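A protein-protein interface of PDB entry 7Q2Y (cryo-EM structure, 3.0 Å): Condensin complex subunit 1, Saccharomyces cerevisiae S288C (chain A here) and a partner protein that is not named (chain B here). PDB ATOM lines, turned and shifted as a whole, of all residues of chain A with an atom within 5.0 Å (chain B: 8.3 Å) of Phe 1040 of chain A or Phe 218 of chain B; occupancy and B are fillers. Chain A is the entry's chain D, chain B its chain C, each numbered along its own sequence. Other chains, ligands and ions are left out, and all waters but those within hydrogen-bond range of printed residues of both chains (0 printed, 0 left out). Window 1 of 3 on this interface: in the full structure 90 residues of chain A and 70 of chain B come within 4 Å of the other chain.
The backbone carbonyl oxygen (O) of Phe 218 of chain B is in hydrogen-bond range of the guanidinium group (NH2) of Arg 1032 of chain A (3.4 Å). The side-chain carboxylate (OD1) of Asp 219 of chain B lies close to the guanidinium group (NH2) of Arg 1032 of chain A (2.3 Å).
N of Phe 188 of chain B is in hydrogen-bond range of O of Ala 220 of chain B (3.5 Å). The side-chain hydroxyl (OG1) of Thr 1037 of chain A is in hydrogen-bond range of the backbone carbonyl oxygen (O) of Thr 1033 of chain A.
CD2 of Leu 999 of chain A touches CD2 of Leu 204 of chain B (3.8 Å). Leu 999 of chain A touches Phe 218 of chain B (CD2 to CD1, 3.9 Å). Phe 218 of chain B touches Met 1036 of chain A (CE2 to CG, 3.4 Å). Met 1036 of chain A touches Ala 220 of chain B. Thr 1037 of chain A touches Phe 218 of chain B. Phe 1040 of chain A touches Phe 188 of chain B (CE1 to CE1, 3.4 Å). CE2 of Phe 195 of chain B touches O of Phe 1040 of chain A, at 3.4 Å. Phe 188 of chain B touches Leu 1043 of chain A (CE2 to CD1, 3.9 Å). CD1 of Leu 1043 of chain A touches CD2 of Leu 192 of chain B (3.6 Å). CB of Ala 1044 of chain A touches CE2 of Phe 195 of chain B, 3.5 Å away.
Printed residues of chain B within 4 Å of Leu 999 of chain A: Leu 204 (3.8 Å), Val 216 (3.7 Å) and Phe 218 (3.9 Å). Of the printed residues of chain B, Thr 1033 of chain A touches Phe 218 (3.9 Å). Of the printed residues of chain B, Phe 1040 of chain A touches Phe 188, Phe 195 and Phe 218. Ile 1042 of chain A touches none of the printed residues of chain B. Of the printed residues of chain A, Phe 188 of chain B touches Phe 1040 (3.4 Å) and Leu 1043 (3.9 Å). Ile 217 of chain B touches none of the printed residues of chain A. Of chain A, only Leu 999, Arg 1032, Thr 1033, Met 1036, Thr 1037 and Phe 1040 come within 4 Å of Phe 218 of chain B. The nearest residue of chain B that does not touch Phe 1040 of chain A is Leu 192 of chain B (4.1 Å). The nearest printed residue of chain B that does not touch Arg 1032 of chain A is Ala 220 of chain B (4.5 Å).
Printed residues of chain A that touch a printed residue of chain B: Leu 999, Arg 1032, Thr 1033, Met 1036, Thr 1037, Phe 1040, Leu 1043 and Ala 1044. Hydrophobic or aromatic side chains of chain A that line the printed part of chain B: Leu 999, Met 1036, Phe 1040, Leu 1043 and Ala 1044. Of the 24 printed residues of chain B, 9 touch a printed residue of chain A. Printed residues of chain B that touch a printed residue of chain A: Phe 188, Leu 192, Phe 195, Asp 196, Leu 204, Val 216, Phe 218, Asp 219 and Ala 220. Hydrophobic or aromatic side chains of chain B that line the printed part of chain A: Phe 188, Leu 192, Phe 195, Leu 204, Val 216, Phe 218 and Ala 220. Among the printed residues, Asp or Glu carboxylates within 4 Å of a Lys or Arg side-chain nitrogen of the other chain: Arg 1032 of chain A with Asp 219 of chain B (2.3 Å).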
ATOM      1  N   LEU A 999      -3.750 -16.951  13.979  1.00  0.00           N
ATOM      2  CA  LEU A 999      -2.993 -16.762  15.217  1.00  0.00           C
ATOM      3  C   LEU A 999      -2.430 -18.084  15.733  1.00  0.00           C
ATOM      4  O   LEU A 999      -1.287 -18.142  16.211  1.00  0.00           O
ATOM      5  CB  LEU A 999      -3.874 -16.100  16.275  1.00  0.00           C
ATOM      6  CG  LEU A 999      -4.170 -14.617  16.045  1.00  0.00           C
ATOM      7  CD1 LEU A 999      -5.239 -14.125  17.004  1.00  0.00           C
ATOM      8  CD2 LEU A 999      -2.903 -13.792  16.183  1.00  0.00           C
ATOM      9  N   ARG A1032      -5.280  -8.233   7.545  1.00  0.00           N
ATOM     10  CA  ARG A1032      -4.410  -7.425   8.395  1.00  0.00           C
ATOM     11  C   ARG A1032      -3.818  -8.244   9.536  1.00  0.00           C
ATOM     12  O   ARG A1032      -2.630  -8.106   9.856  1.00  0.00           O
ATOM     13  CB  ARG A1032      -5.189  -6.229   8.945  1.00  0.00           C
ATOM     14  CG  ARG A1032      -4.672  -5.712  10.280  1.00  0.00           C
ATOM     15  CD  ARG A1032      -5.354  -4.409  10.687  1.00  0.00           C
ATOM     16  NE  ARG A1032      -4.994  -3.967  12.031  1.00  0.00           N
ATOM     17  CZ  ARG A1032      -5.205  -4.656  13.147  1.00  0.00           C
ATOM     18  NH1 ARG A1032      -5.842  -5.816  13.138  1.00  0.00           N
ATOM     19  NH2 ARG A1032      -4.783  -4.158  14.306  1.00  0.00           N
ATOM     20  N   THR A1033      -4.633  -9.087  10.176  1.00  0.00           N
ATOM     21  CA  THR A1033      -4.115  -9.941  11.240  1.00  0.00           C
ATOM     22  C   THR A1033      -3.048 -10.888  10.710  1.00  0.00           C
ATOM     23  O   THR A1033      -2.001 -11.069  11.341  1.00  0.00           O
ATOM     24  CB  THR A1033      -5.253 -10.726  11.897  1.00  0.00           C
ATOM     25  OG1 THR A1033      -6.031 -11.383  10.889  1.00  0.00           O
ATOM     26  CG2 THR A1033      -6.145  -9.801  12.714  1.00  0.00           C
ATOM     27  N   MET A1036       0.172  -8.896  10.051  1.00  0.00           N
ATOM     28  CA  MET A1036       0.921  -8.512  11.243  1.00  0.00           C
ATOM     29  C   MET A1036       1.534  -9.736  11.921  1.00  0.00           C
ATOM     30  O   MET A1036       2.636  -9.658  12.480  1.00  0.00           O
ATOM     31  CB  MET A1036       0.028  -7.727  12.203  1.00  0.00           C
ATOM     32  CG  MET A1036       0.764  -7.178  13.418  1.00  0.00           C
ATOM     33  SD  MET A1036      -0.304  -6.242  14.529  1.00  0.00           S
ATOM     34  CE  MET A1036      -0.583  -4.759  13.565  1.00  0.00           C
ATOM     35  N   THR A1037       0.864 -10.890  11.839  1.00  0.00           N
ATOM     36  CA  THR A1037       1.454 -12.122  12.358  1.00  0.00           C
ATOM     37  C   THR A1037       2.719 -12.492  11.591  1.00  0.00           C
ATOM     38  O   THR A1037       3.750 -12.828  12.190  1.00  0.00           O
ATOM     39  CB  THR A1037       0.433 -13.259  12.294  1.00  0.00           C
ATOM     40  OG1 THR A1037      -0.689 -12.946  13.128  1.00  0.00           O
ATOM     41  CG2 THR A1037       1.057 -14.563  12.765  1.00  0.00           C
ATOM     42  N   VAL A1038       2.663 -12.433  10.257  1.00  0.00           N
ATOM     43  CA  VAL A1038       3.857 -12.770   9.486  1.00  0.00           C
ATOM     44  C   VAL A1038       4.932 -11.705   9.675  1.00  0.00           C
ATOM     45  O   VAL A1038       6.127 -12.015   9.640  1.00  0.00           O
ATOM     46  CB  VAL A1038       3.525 -13.002   7.997  1.00  0.00           C
ATOM     47  CG1 VAL A1038       2.482 -14.101   7.850  1.00  0.00           C
ATOM     48  CG2 VAL A1038       3.074 -11.727   7.314  1.00  0.00           C
ATOM     49  N   THR A1039       4.541 -10.450   9.918  1.00  0.00           N
ATOM     50  CA  THR A1039       5.518  -9.411  10.229  1.00  0.00           C
ATOM     51  C   THR A1039       6.261  -9.725  11.519  1.00  0.00           C
ATOM     52  O   THR A1039       7.491  -9.622  11.582  1.00  0.00           O
ATOM     53  CB  THR A1039       4.821  -8.053  10.334  1.00  0.00           C
ATOM     54  OG1 THR A1039       4.000  -7.841   9.179  1.00  0.00           O
ATOM     55  CG2 THR A1039       5.843  -6.932  10.445  1.00  0.00           C
ATOM     56  N   PHE A1040       5.521 -10.097  12.567  1.00  0.00           N
ATOM     57  CA  PHE A1040       6.159 -10.485  13.823  1.00  0.00           C
ATOM     58  C   PHE A1040       7.073 -11.685  13.626  1.00  0.00           C
ATOM     59  O   PHE A1040       8.188 -11.720  14.160  1.00  0.00           O
ATOM     60  CB  PHE A1040       5.107 -10.789  14.891  1.00  0.00           C
ATOM     61  CG  PHE A1040       4.473  -9.567  15.488  1.00  0.00           C
ATOM     62  CD1 PHE A1040       5.059  -8.322  15.337  1.00  0.00           C
ATOM     63  CD2 PHE A1040       3.304  -9.666  16.222  1.00  0.00           C
ATOM     64  CE1 PHE A1040       4.482  -7.199  15.893  1.00  0.00           C
ATOM     65  CE2 PHE A1040       2.723  -8.544  16.781  1.00  0.00           C
ATOM     66  CZ  PHE A1040       3.313  -7.309  16.615  1.00  0.00           C
ATOM     67  N   LEU A1041       6.618 -12.679  12.860  1.00  0.00           N
ATOM     68  CA  LEU A1041       7.444 -13.857  12.614  1.00  0.00           C
ATOM     69  C   LEU A1041       8.738 -13.490  11.894  1.00  0.00           C
ATOM     70  O   LEU A1041       9.821 -13.954  12.273  1.00  0.00           O
ATOM     71  CB  LEU A1041       6.659 -14.895  11.814  1.00  0.00           C
ATOM     72  CG  LEU A1041       5.639 -15.714  12.605  1.00  0.00           C
ATOM     73  CD1 LEU A1041       4.743 -16.502  11.669  1.00  0.00           C
ATOM     74  CD2 LEU A1041       6.343 -16.639  13.580  1.00  0.00           C
ATOM     75  N   ILE A1042       8.648 -12.645  10.865  1.00  0.00           N
ATOM     76  CA  ILE A1042       9.834 -12.247  10.114  1.00  0.00           C
ATOM     77  C   ILE A1042      10.787 -11.450  10.994  1.00  0.00           C
ATOM     78  O   ILE A1042      12.005 -11.665  10.964  1.00  0.00           O
ATOM     79  CB  ILE A1042       9.426 -11.461   8.855  1.00  0.00           C
ATOM     80  CG1 ILE A1042       8.786 -12.398   7.831  1.00  0.00           C
ATOM     81  CG2 ILE A1042      10.627 -10.752   8.250  1.00  0.00           C
ATOM     82  CD1 ILE A1042       8.072 -11.678   6.711  1.00  0.00           C
ATOM     83  N   LEU A1043      10.258 -10.522  11.797  1.00  0.00           N
ATOM     84  CA  LEU A1043      11.124  -9.722  12.655  1.00  0.00           C
ATOM     85  C   LEU A1043      11.790 -10.572  13.729  1.00  0.00           C
ATOM     86  O   LEU A1043      12.934 -10.299  14.109  1.00  0.00           O
ATOM     87  CB  LEU A1043      10.336  -8.577  13.294  1.00  0.00           C
ATOM     88  CG  LEU A1043       9.658  -7.584  12.343  1.00  0.00           C
ATOM     89  CD1 LEU A1043       9.231  -6.321  13.076  1.00  0.00           C
ATOM     90  CD2 LEU A1043      10.545  -7.251  11.157  1.00  0.00           C
ATOM     91  N   ALA A1044      11.099 -11.599  14.231  1.00  0.00           N
ATOM     92  CA  ALA A1044      11.729 -12.507  15.183  1.00  0.00           C
ATOM     93  C   ALA A1044      12.781 -13.380  14.511  1.00  0.00           C
ATOM     94  O   ALA A1044      13.804 -13.699  15.128  1.00  0.00           O
ATOM     95  CB  ALA A1044      10.673 -13.377  15.863  1.00  0.00           C
ATOM     96  N   GLY A1045      12.552 -13.772  13.262  1.00  0.00           N
ATOM     97  CA  GLY A1045      13.489 -14.608  12.544  1.00  0.00           C
ATOM     98  C   GLY A1045      13.147 -16.079  12.507  1.00  0.00           C
ATOM     99  O   GLY A1045      13.978 -16.876  12.057  1.00  0.00           O
ATOM    100  N   LEU B 187       3.944   1.068  20.955  1.00  0.00           N
ATOM    101  CA  LEU B 187       3.251  -0.170  21.297  1.00  0.00           C
ATOM    102  C   LEU B 187       3.688  -1.315  20.393  1.00  0.00           C
ATOM    103  O   LEU B 187       3.771  -2.466  20.839  1.00  0.00           O
ATOM    104  CB  LEU B 187       1.739   0.028  21.229  1.00  0.00           C
ATOM    105  CG  LEU B 187       1.134   0.897  22.334  1.00  0.00           C
ATOM    106  CD1 LEU B 187      -0.334   0.567  22.503  1.00  0.00           C
ATOM    107  CD2 LEU B 187       1.880   0.718  23.648  1.00  0.00           C
ATOM    108  N   PHE B 188       3.967  -1.022  19.121  1.00  0.00           N
ATOM    109  CA  PHE B 188       4.516  -2.045  18.237  1.00  0.00           C
ATOM    110  C   PHE B 188       5.861  -2.539  18.752  1.00  0.00           C
ATOM    111  O   PHE B 188       6.133  -3.744  18.741  1.00  0.00           O
ATOM    112  CB  PHE B 188       4.652  -1.497  16.817  1.00  0.00           C
ATOM    113  CG  PHE B 188       5.021  -2.533  15.795  1.00  0.00           C
ATOM    114  CD1 PHE B 188       4.046  -3.316  15.202  1.00  0.00           C
ATOM    115  CD2 PHE B 188       6.341  -2.722  15.422  1.00  0.00           C
ATOM    116  CE1 PHE B 188       4.379  -4.266  14.258  1.00  0.00           C
ATOM    117  CE2 PHE B 188       6.681  -3.673  14.481  1.00  0.00           C
ATOM    118  CZ  PHE B 188       5.698  -4.446  13.898  1.00  0.00           C
ATOM    119  N   LYS B 189       6.712  -1.620  19.216  1.00  0.00           N
ATOM    120  CA  LYS B 189       8.001  -2.012  19.777  1.00  0.00           C
ATOM    121  C   LYS B 189       7.826  -2.869  21.026  1.00  0.00           C
ATOM    122  O   LYS B 189       8.527  -3.873  21.201  1.00  0.00           O
ATOM    123  CB  LYS B 189       8.832  -0.769  20.094  1.00  0.00           C
ATOM    124  CG  LYS B 189      10.232  -1.060  20.608  1.00  0.00           C
ATOM    125  CD  LYS B 189      11.001   0.231  20.845  1.00  0.00           C
ATOM    126  CE  LYS B 189      12.434  -0.047  21.270  1.00  0.00           C
ATOM    127  NZ  LYS B 189      12.501  -0.677  22.617  1.00  0.00           N
ATOM    128  N   LYS B 190       6.899  -2.486  21.907  1.00  0.00           N
ATOM    129  CA  LYS B 190       6.668  -3.263  23.123  1.00  0.00           C
ATOM    130  C   LYS B 190       6.166  -4.664  22.793  1.00  0.00           C
ATOM    131  O   LYS B 190       6.637  -5.659  23.362  1.00  0.00           O
ATOM    132  CB  LYS B 190       5.669  -2.539  24.026  1.00  0.00           C
ATOM    133  CG  LYS B 190       5.396  -3.255  25.338  1.00  0.00           C
ATOM    134  CD  LYS B 190       4.501  -2.431  26.245  1.00  0.00           C
ATOM    135  CE  LYS B 190       3.070  -2.423  25.734  1.00  0.00           C
ATOM    136  NZ  LYS B 190       2.144  -1.720  26.664  1.00  0.00           N
ATOM    137  N   ALA B 191       5.206  -4.760  21.870  1.00  0.00           N
ATOM    138  CA  ALA B 191       4.681  -6.062  21.474  1.00  0.00           C
ATOM    139  C   ALA B 191       5.762  -6.910  20.819  1.00  0.00           C
ATOM    140  O   ALA B 191       5.843  -8.118  21.062  1.00  0.00           O
ATOM    141  CB  ALA B 191       3.490  -5.886  20.534  1.00  0.00           C
ATOM    142  N   LEU B 192       6.605  -6.293  19.988  1.00  0.00           N
ATOM    143  CA  LEU B 192       7.686  -7.026  19.342  1.00  0.00           C
ATOM    144  C   LEU B 192       8.695  -7.539  20.361  1.00  0.00           C
ATOM    145  O   LEU B 192       9.173  -8.672  20.248  1.00  0.00           O
ATOM    146  CB  LEU B 192       8.366  -6.134  18.306  1.00  0.00           C
ATOM    147  CG  LEU B 192       9.465  -6.763  17.452  1.00  0.00           C
ATOM    148  CD1 LEU B 192       8.914  -7.922  16.643  1.00  0.00           C
ATOM    149  CD2 LEU B 192      10.071  -5.710  16.542  1.00  0.00           C
ATOM    150  N   VAL B 193       9.030  -6.723  21.364  1.00  0.00           N
ATOM    151  CA  VAL B 193       9.967  -7.162  22.396  1.00  0.00           C
ATOM    152  C   VAL B 193       9.378  -8.319  23.195  1.00  0.00           C
ATOM    153  O   VAL B 193      10.053  -9.326  23.450  1.00  0.00           O
ATOM    154  CB  VAL B 193      10.350  -5.979  23.306  1.00  0.00           C
ATOM    155  CG1 VAL B 193      11.024  -6.478  24.575  1.00  0.00           C
ATOM    156  CG2 VAL B 193      11.258  -5.013  22.562  1.00  0.00           C
ATOM    157  N   PHE B 195       7.086 -10.431  22.222  1.00  0.00           N
ATOM    158  CA  PHE B 195       7.035 -11.586  21.334  1.00  0.00           C
ATOM    159  C   PHE B 195       8.408 -12.227  21.173  1.00  0.00           C
ATOM    160  O   PHE B 195       8.529 -13.457  21.155  1.00  0.00           O
ATOM    161  CB  PHE B 195       6.474 -11.148  19.982  1.00  0.00           C
ATOM    162  CG  PHE B 195       6.421 -12.237  18.956  1.00  0.00           C
ATOM    163  CD1 PHE B 195       5.408 -13.177  18.971  1.00  0.00           C
ATOM    164  CD2 PHE B 195       7.377 -12.302  17.956  1.00  0.00           C
ATOM    165  CE1 PHE B 195       5.358 -14.170  18.018  1.00  0.00           C
ATOM    166  CE2 PHE B 195       7.330 -13.292  17.002  1.00  0.00           C
ATOM    167  CZ  PHE B 195       6.321 -14.223  17.031  1.00  0.00           C
ATOM    168  N   ASP B 196       9.455 -11.408  21.055  1.00  0.00           N
ATOM    169  CA  ASP B 196      10.803 -11.928  20.874  1.00  0.00           C
ATOM    170  C   ASP B 196      11.396 -12.470  22.166  1.00  0.00           C
ATOM    171  O   ASP B 196      12.427 -13.152  22.117  1.00  0.00           O
ATOM    172  CB  ASP B 196      11.713 -10.840  20.302  1.00  0.00           C
ATOM    173  CG  ASP B 196      12.901 -11.410  19.555  1.00  0.00           C
ATOM    174  OD1 ASP B 196      12.691 -12.230  18.637  1.00  0.00           O
ATOM    175  OD2 ASP B 196      14.045 -11.041  19.890  1.00  0.00           O
ATOM    176  N   LEU B 203       2.899 -16.516  23.929  1.00  0.00           N
ATOM    177  CA  LEU B 203       2.389 -17.388  22.879  1.00  0.00           C
ATOM    178  C   LEU B 203       1.440 -16.687  21.918  1.00  0.00           C
ATOM    179  O   LEU B 203       0.919 -17.342  21.010  1.00  0.00           O
ATOM    180  CB  LEU B 203       1.677 -18.592  23.501  1.00  0.00           C
ATOM    181  CG  LEU B 203       2.525 -19.547  24.340  1.00  0.00           C
ATOM    182  CD1 LEU B 203       1.649 -20.609  24.986  1.00  0.00           C
ATOM    183  CD2 LEU B 203       3.610 -20.189  23.491  1.00  0.00           C
ATOM    184  N   LEU B 204       1.169 -15.396  22.109  1.00  0.00           N
ATOM    185  CA  LEU B 204       0.253 -14.606  21.292  1.00  0.00           C
ATOM    186  C   LEU B 204      -1.186 -15.089  21.421  1.00  0.00           C
ATOM    187  O   LEU B 204      -2.076 -14.522  20.780  1.00  0.00           O
ATOM    188  CB  LEU B 204       0.657 -14.588  19.810  1.00  0.00           C
ATOM    189  CG  LEU B 204       0.360 -13.328  18.997  1.00  0.00           C
ATOM    190  CD1 LEU B 204       1.189 -12.159  19.504  1.00  0.00           C
ATOM    191  CD2 LEU B 204       0.633 -13.582  17.524  1.00  0.00           C
ATOM    192  N   LEU B 205      -1.444 -16.125  22.220  1.00  0.00           N
ATOM    193  CA  LEU B 205      -2.794 -16.553  22.549  1.00  0.00           C
ATOM    194  C   LEU B 205      -3.159 -16.266  23.997  1.00  0.00           C
ATOM    195  O   LEU B 205      -4.349 -16.273  24.333  1.00  0.00           O
ATOM    196  CB  LEU B 205      -2.962 -18.055  22.270  1.00  0.00           C
ATOM    197  CG  LEU B 205      -3.301 -18.442  20.829  1.00  0.00           C
ATOM    198  CD1 LEU B 205      -3.093 -19.931  20.609  1.00  0.00           C
ATOM    199  CD2 LEU B 205      -4.727 -18.041  20.487  1.00  0.00           C
ATOM    200  N   THR B 207      -1.215 -13.525  25.789  1.00  0.00           N
ATOM    201  CA  THR B 207      -0.998 -12.087  25.911  1.00  0.00           C
ATOM    202  C   THR B 207      -2.185 -11.301  25.370  1.00  0.00           C
ATOM    203  O   THR B 207      -2.581 -10.281  25.945  1.00  0.00           O
ATOM    204  CB  THR B 207       0.285 -11.686  25.181  1.00  0.00           C
ATOM    205  OG1 THR B 207       1.353 -12.557  25.575  1.00  0.00           O
ATOM    206  CG2 THR B 207       0.663 -10.250  25.515  1.00  0.00           C
ATOM    207  N   LEU B 208      -2.768 -11.761  24.266  1.00  0.00           N
ATOM    208  CA  LEU B 208      -3.898 -11.073  23.668  1.00  0.00           C
ATOM    209  C   LEU B 208      -5.156 -11.265  24.513  1.00  0.00           C
ATOM    210  O   LEU B 208      -5.203 -12.072  25.446  1.00  0.00           O
ATOM    211  CB  LEU B 208      -4.141 -11.572  22.247  1.00  0.00           C
ATOM    212  CG  LEU B 208      -3.009 -11.391  21.239  1.00  0.00           C
ATOM    213  CD1 LEU B 208      -3.467 -11.862  19.874  1.00  0.00           C
ATOM    214  CD2 LEU B 208      -2.552  -9.943  21.186  1.00  0.00           C
ATOM    215  N   ASN B 209      -6.192 -10.504  24.168  1.00  0.00           N
ATOM    216  CA  ASN B 209      -7.464 -10.539  24.869  1.00  0.00           C
ATOM    217  C   ASN B 209      -8.571 -10.967  23.914  1.00  0.00           C
ATOM    218  O   ASN B 209      -8.555 -10.629  22.727  1.00  0.00           O
ATOM    219  CB  ASN B 209      -7.800  -9.174  25.478  1.00  0.00           C
ATOM    220  CG  ASN B 209      -6.828  -8.769  26.568  1.00  0.00           C
ATOM    221  OD1 ASN B 209      -6.406  -9.593  27.379  1.00  0.00           O
ATOM    222  ND2 ASN B 209      -6.464  -7.492  26.592  1.00  0.00           N
ATOM    223  N   ILE B 210      -9.529 -11.712  24.445  1.00  0.00           N
ATOM    224  CA  ILE B 210     -10.666 -12.202  23.675  1.00  0.00           C
ATOM    225  C   ILE B 210     -11.756 -11.138  23.679  1.00  0.00           C
ATOM    226  O   ILE B 210     -11.871 -10.337  24.612  1.00  0.00           O
ATOM    227  CB  ILE B 210     -11.167 -13.550  24.238  1.00  0.00           C
ATOM    228  CG1 ILE B 210     -12.102 -14.248  23.249  1.00  0.00           C
ATOM    229  CG2 ILE B 210     -11.841 -13.357  25.583  1.00  0.00           C
ATOM    230  CD1 ILE B 210     -11.398 -14.787  22.030  1.00  0.00           C
ATOM    231  N   ASP B 211     -12.557 -11.118  22.619  1.00  0.00           N
ATOM    232  CA  ASP B 211     -13.604 -10.126  22.425  1.00  0.00           C
ATOM    233  C   ASP B 211     -14.963 -10.770  22.702  1.00  0.00           C
ATOM    234  O   ASP B 211     -15.058 -11.943  23.075  1.00  0.00           O
ATOM    235  CB  ASP B 211     -13.512  -9.545  21.006  1.00  0.00           C
ATOM    236  CG  ASP B 211     -14.427  -8.349  20.787  1.00  0.00           C
ATOM    237  OD1 ASP B 211     -15.166  -7.974  21.720  1.00  0.00           O
ATOM    238  OD2 ASP B 211     -14.403  -7.783  19.673  1.00  0.00           O
ATOM    239  N   ARG B 215     -13.514 -13.493  19.438  1.00  0.00           N
ATOM    240  CA  ARG B 215     -12.455 -13.055  18.541  1.00  0.00           C
ATOM    241  C   ARG B 215     -11.258 -12.601  19.361  1.00  0.00           C
ATOM    242  O   ARG B 215     -11.402 -11.791  20.284  1.00  0.00           O
ATOM    243  CB  ARG B 215     -12.941 -11.922  17.636  1.00  0.00           C
ATOM    244  CG  ARG B 215     -11.883 -11.394  16.688  1.00  0.00           C
ATOM    245  CD  ARG B 215     -12.476 -10.410  15.700  1.00  0.00           C
ATOM    246  NE  ARG B 215     -12.502  -9.047  16.217  1.00  0.00           N
ATOM    247  CZ  ARG B 215     -11.515  -8.171  16.082  1.00  0.00           C
ATOM    248  NH1 ARG B 215     -10.376  -8.498  15.495  1.00  0.00           N
ATOM    249  NH2 ARG B 215     -11.673  -6.938  16.552  1.00  0.00           N
ATOM    250  N   VAL B 216     -10.082 -13.123  19.027  1.00  0.00           N
ATOM    251  CA  VAL B 216      -8.861 -12.787  19.751  1.00  0.00           C
ATOM    252  C   VAL B 216      -8.356 -11.449  19.219  1.00  0.00           C
ATOM    253  O   VAL B 216      -7.928 -11.349  18.067  1.00  0.00           O
ATOM    254  CB  VAL B 216      -7.801 -13.882  19.603  1.00  0.00           C
ATOM    255  CG1 VAL B 216      -6.580 -13.550  20.436  1.00  0.00           C
ATOM    256  CG2 VAL B 216      -8.372 -15.234  20.003  1.00  0.00           C
ATOM    257  N   ILE B 217      -8.412 -10.415  20.059  1.00  0.00           N
ATOM    258  CA  ILE B 217      -8.000  -9.081  19.639  1.00  0.00           C
ATOM    259  C   ILE B 217      -6.493  -9.060  19.427  1.00  0.00           C
ATOM    260  O   ILE B 217      -5.718  -9.444  20.313  1.00  0.00           O
ATOM    261  CB  ILE B 217      -8.431  -8.032  20.675  1.00  0.00           C
ATOM    262  CG1 ILE B 217      -9.949  -8.052  20.853  1.00  0.00           C
ATOM    263  CG2 ILE B 217      -7.962  -6.647  20.257  1.00  0.00           C
ATOM    264  CD1 ILE B 217     -10.710  -7.709  19.597  1.00  0.00           C
ATOM    265  N   PHE B 218      -6.072  -8.605  18.248  1.00  0.00           N
ATOM    266  CA  PHE B 218      -4.662  -8.562  17.861  1.00  0.00           C
ATOM    267  C   PHE B 218      -4.391  -7.204  17.218  1.00  0.00           C
ATOM    268  O   PHE B 218      -4.482  -7.050  15.997  1.00  0.00           O
ATOM    269  CB  PHE B 218      -4.333  -9.729  16.932  1.00  0.00           C
ATOM    270  CG  PHE B 218      -2.895  -9.790  16.509  1.00  0.00           C
ATOM    271  CD1 PHE B 218      -1.916 -10.232  17.381  1.00  0.00           C
ATOM    272  CD2 PHE B 218      -2.531  -9.463  15.218  1.00  0.00           C
ATOM    273  CE1 PHE B 218      -0.597 -10.303  16.989  1.00  0.00           C
ATOM    274  CE2 PHE B 218      -1.216  -9.543  14.819  1.00  0.00           C
ATOM    275  CZ  PHE B 218      -0.247  -9.960  15.704  1.00  0.00           C
ATOM    276  N   ASP B 219      -4.061  -6.219  18.052  1.00  0.00           N
ATOM    277  CA  ASP B 219      -3.802  -4.852  17.618  1.00  0.00           C
ATOM    278  C   ASP B 219      -2.513  -4.368  18.263  1.00  0.00           C
ATOM    279  O   ASP B 219      -2.324  -4.526  19.474  1.00  0.00           O
ATOM    280  CB  ASP B 219      -4.968  -3.931  17.985  1.00  0.00           C
ATOM    281  CG  ASP B 219      -4.922  -2.608  17.246  1.00  0.00           C
ATOM    282  OD1 ASP B 219      -4.642  -2.613  16.030  1.00  0.00           O
ATOM    283  OD2 ASP B 219      -5.165  -1.562  17.883  1.00  0.00           O
ATOM    284  N   ALA B 220      -1.628  -3.776  17.454  1.00  0.00           N
ATOM    285  CA  ALA B 220      -0.364  -3.243  17.946  1.00  0.00           C
ATOM    286  C   ALA B 220      -0.055  -1.874  17.351  1.00  0.00           C
ATOM    287  O   ALA B 220       1.120  -1.524  17.192  1.00  0.00           O
ATOM    288  CB  ALA B 220       0.784  -4.214  17.660  1.00  0.00           C
ATOM    289  N   SER B 221      -1.079  -1.093  17.018  1.00  0.00           N
ATOM    290  CA  SER B 221      -0.912   0.215  16.402  1.00  0.00           C
ATOM    291  C   SER B 221      -1.424   1.298  17.341  1.00  0.00           C
ATOM    292  O   SER B 221      -2.420   1.104  18.045  1.00  0.00           O
ATOM    293  CB  SER B 221      -1.649   0.294  15.061  1.00  0.00           C
ATOM    294  OG  SER B 221      -3.017   0.613  15.249  1.00  0.00           O
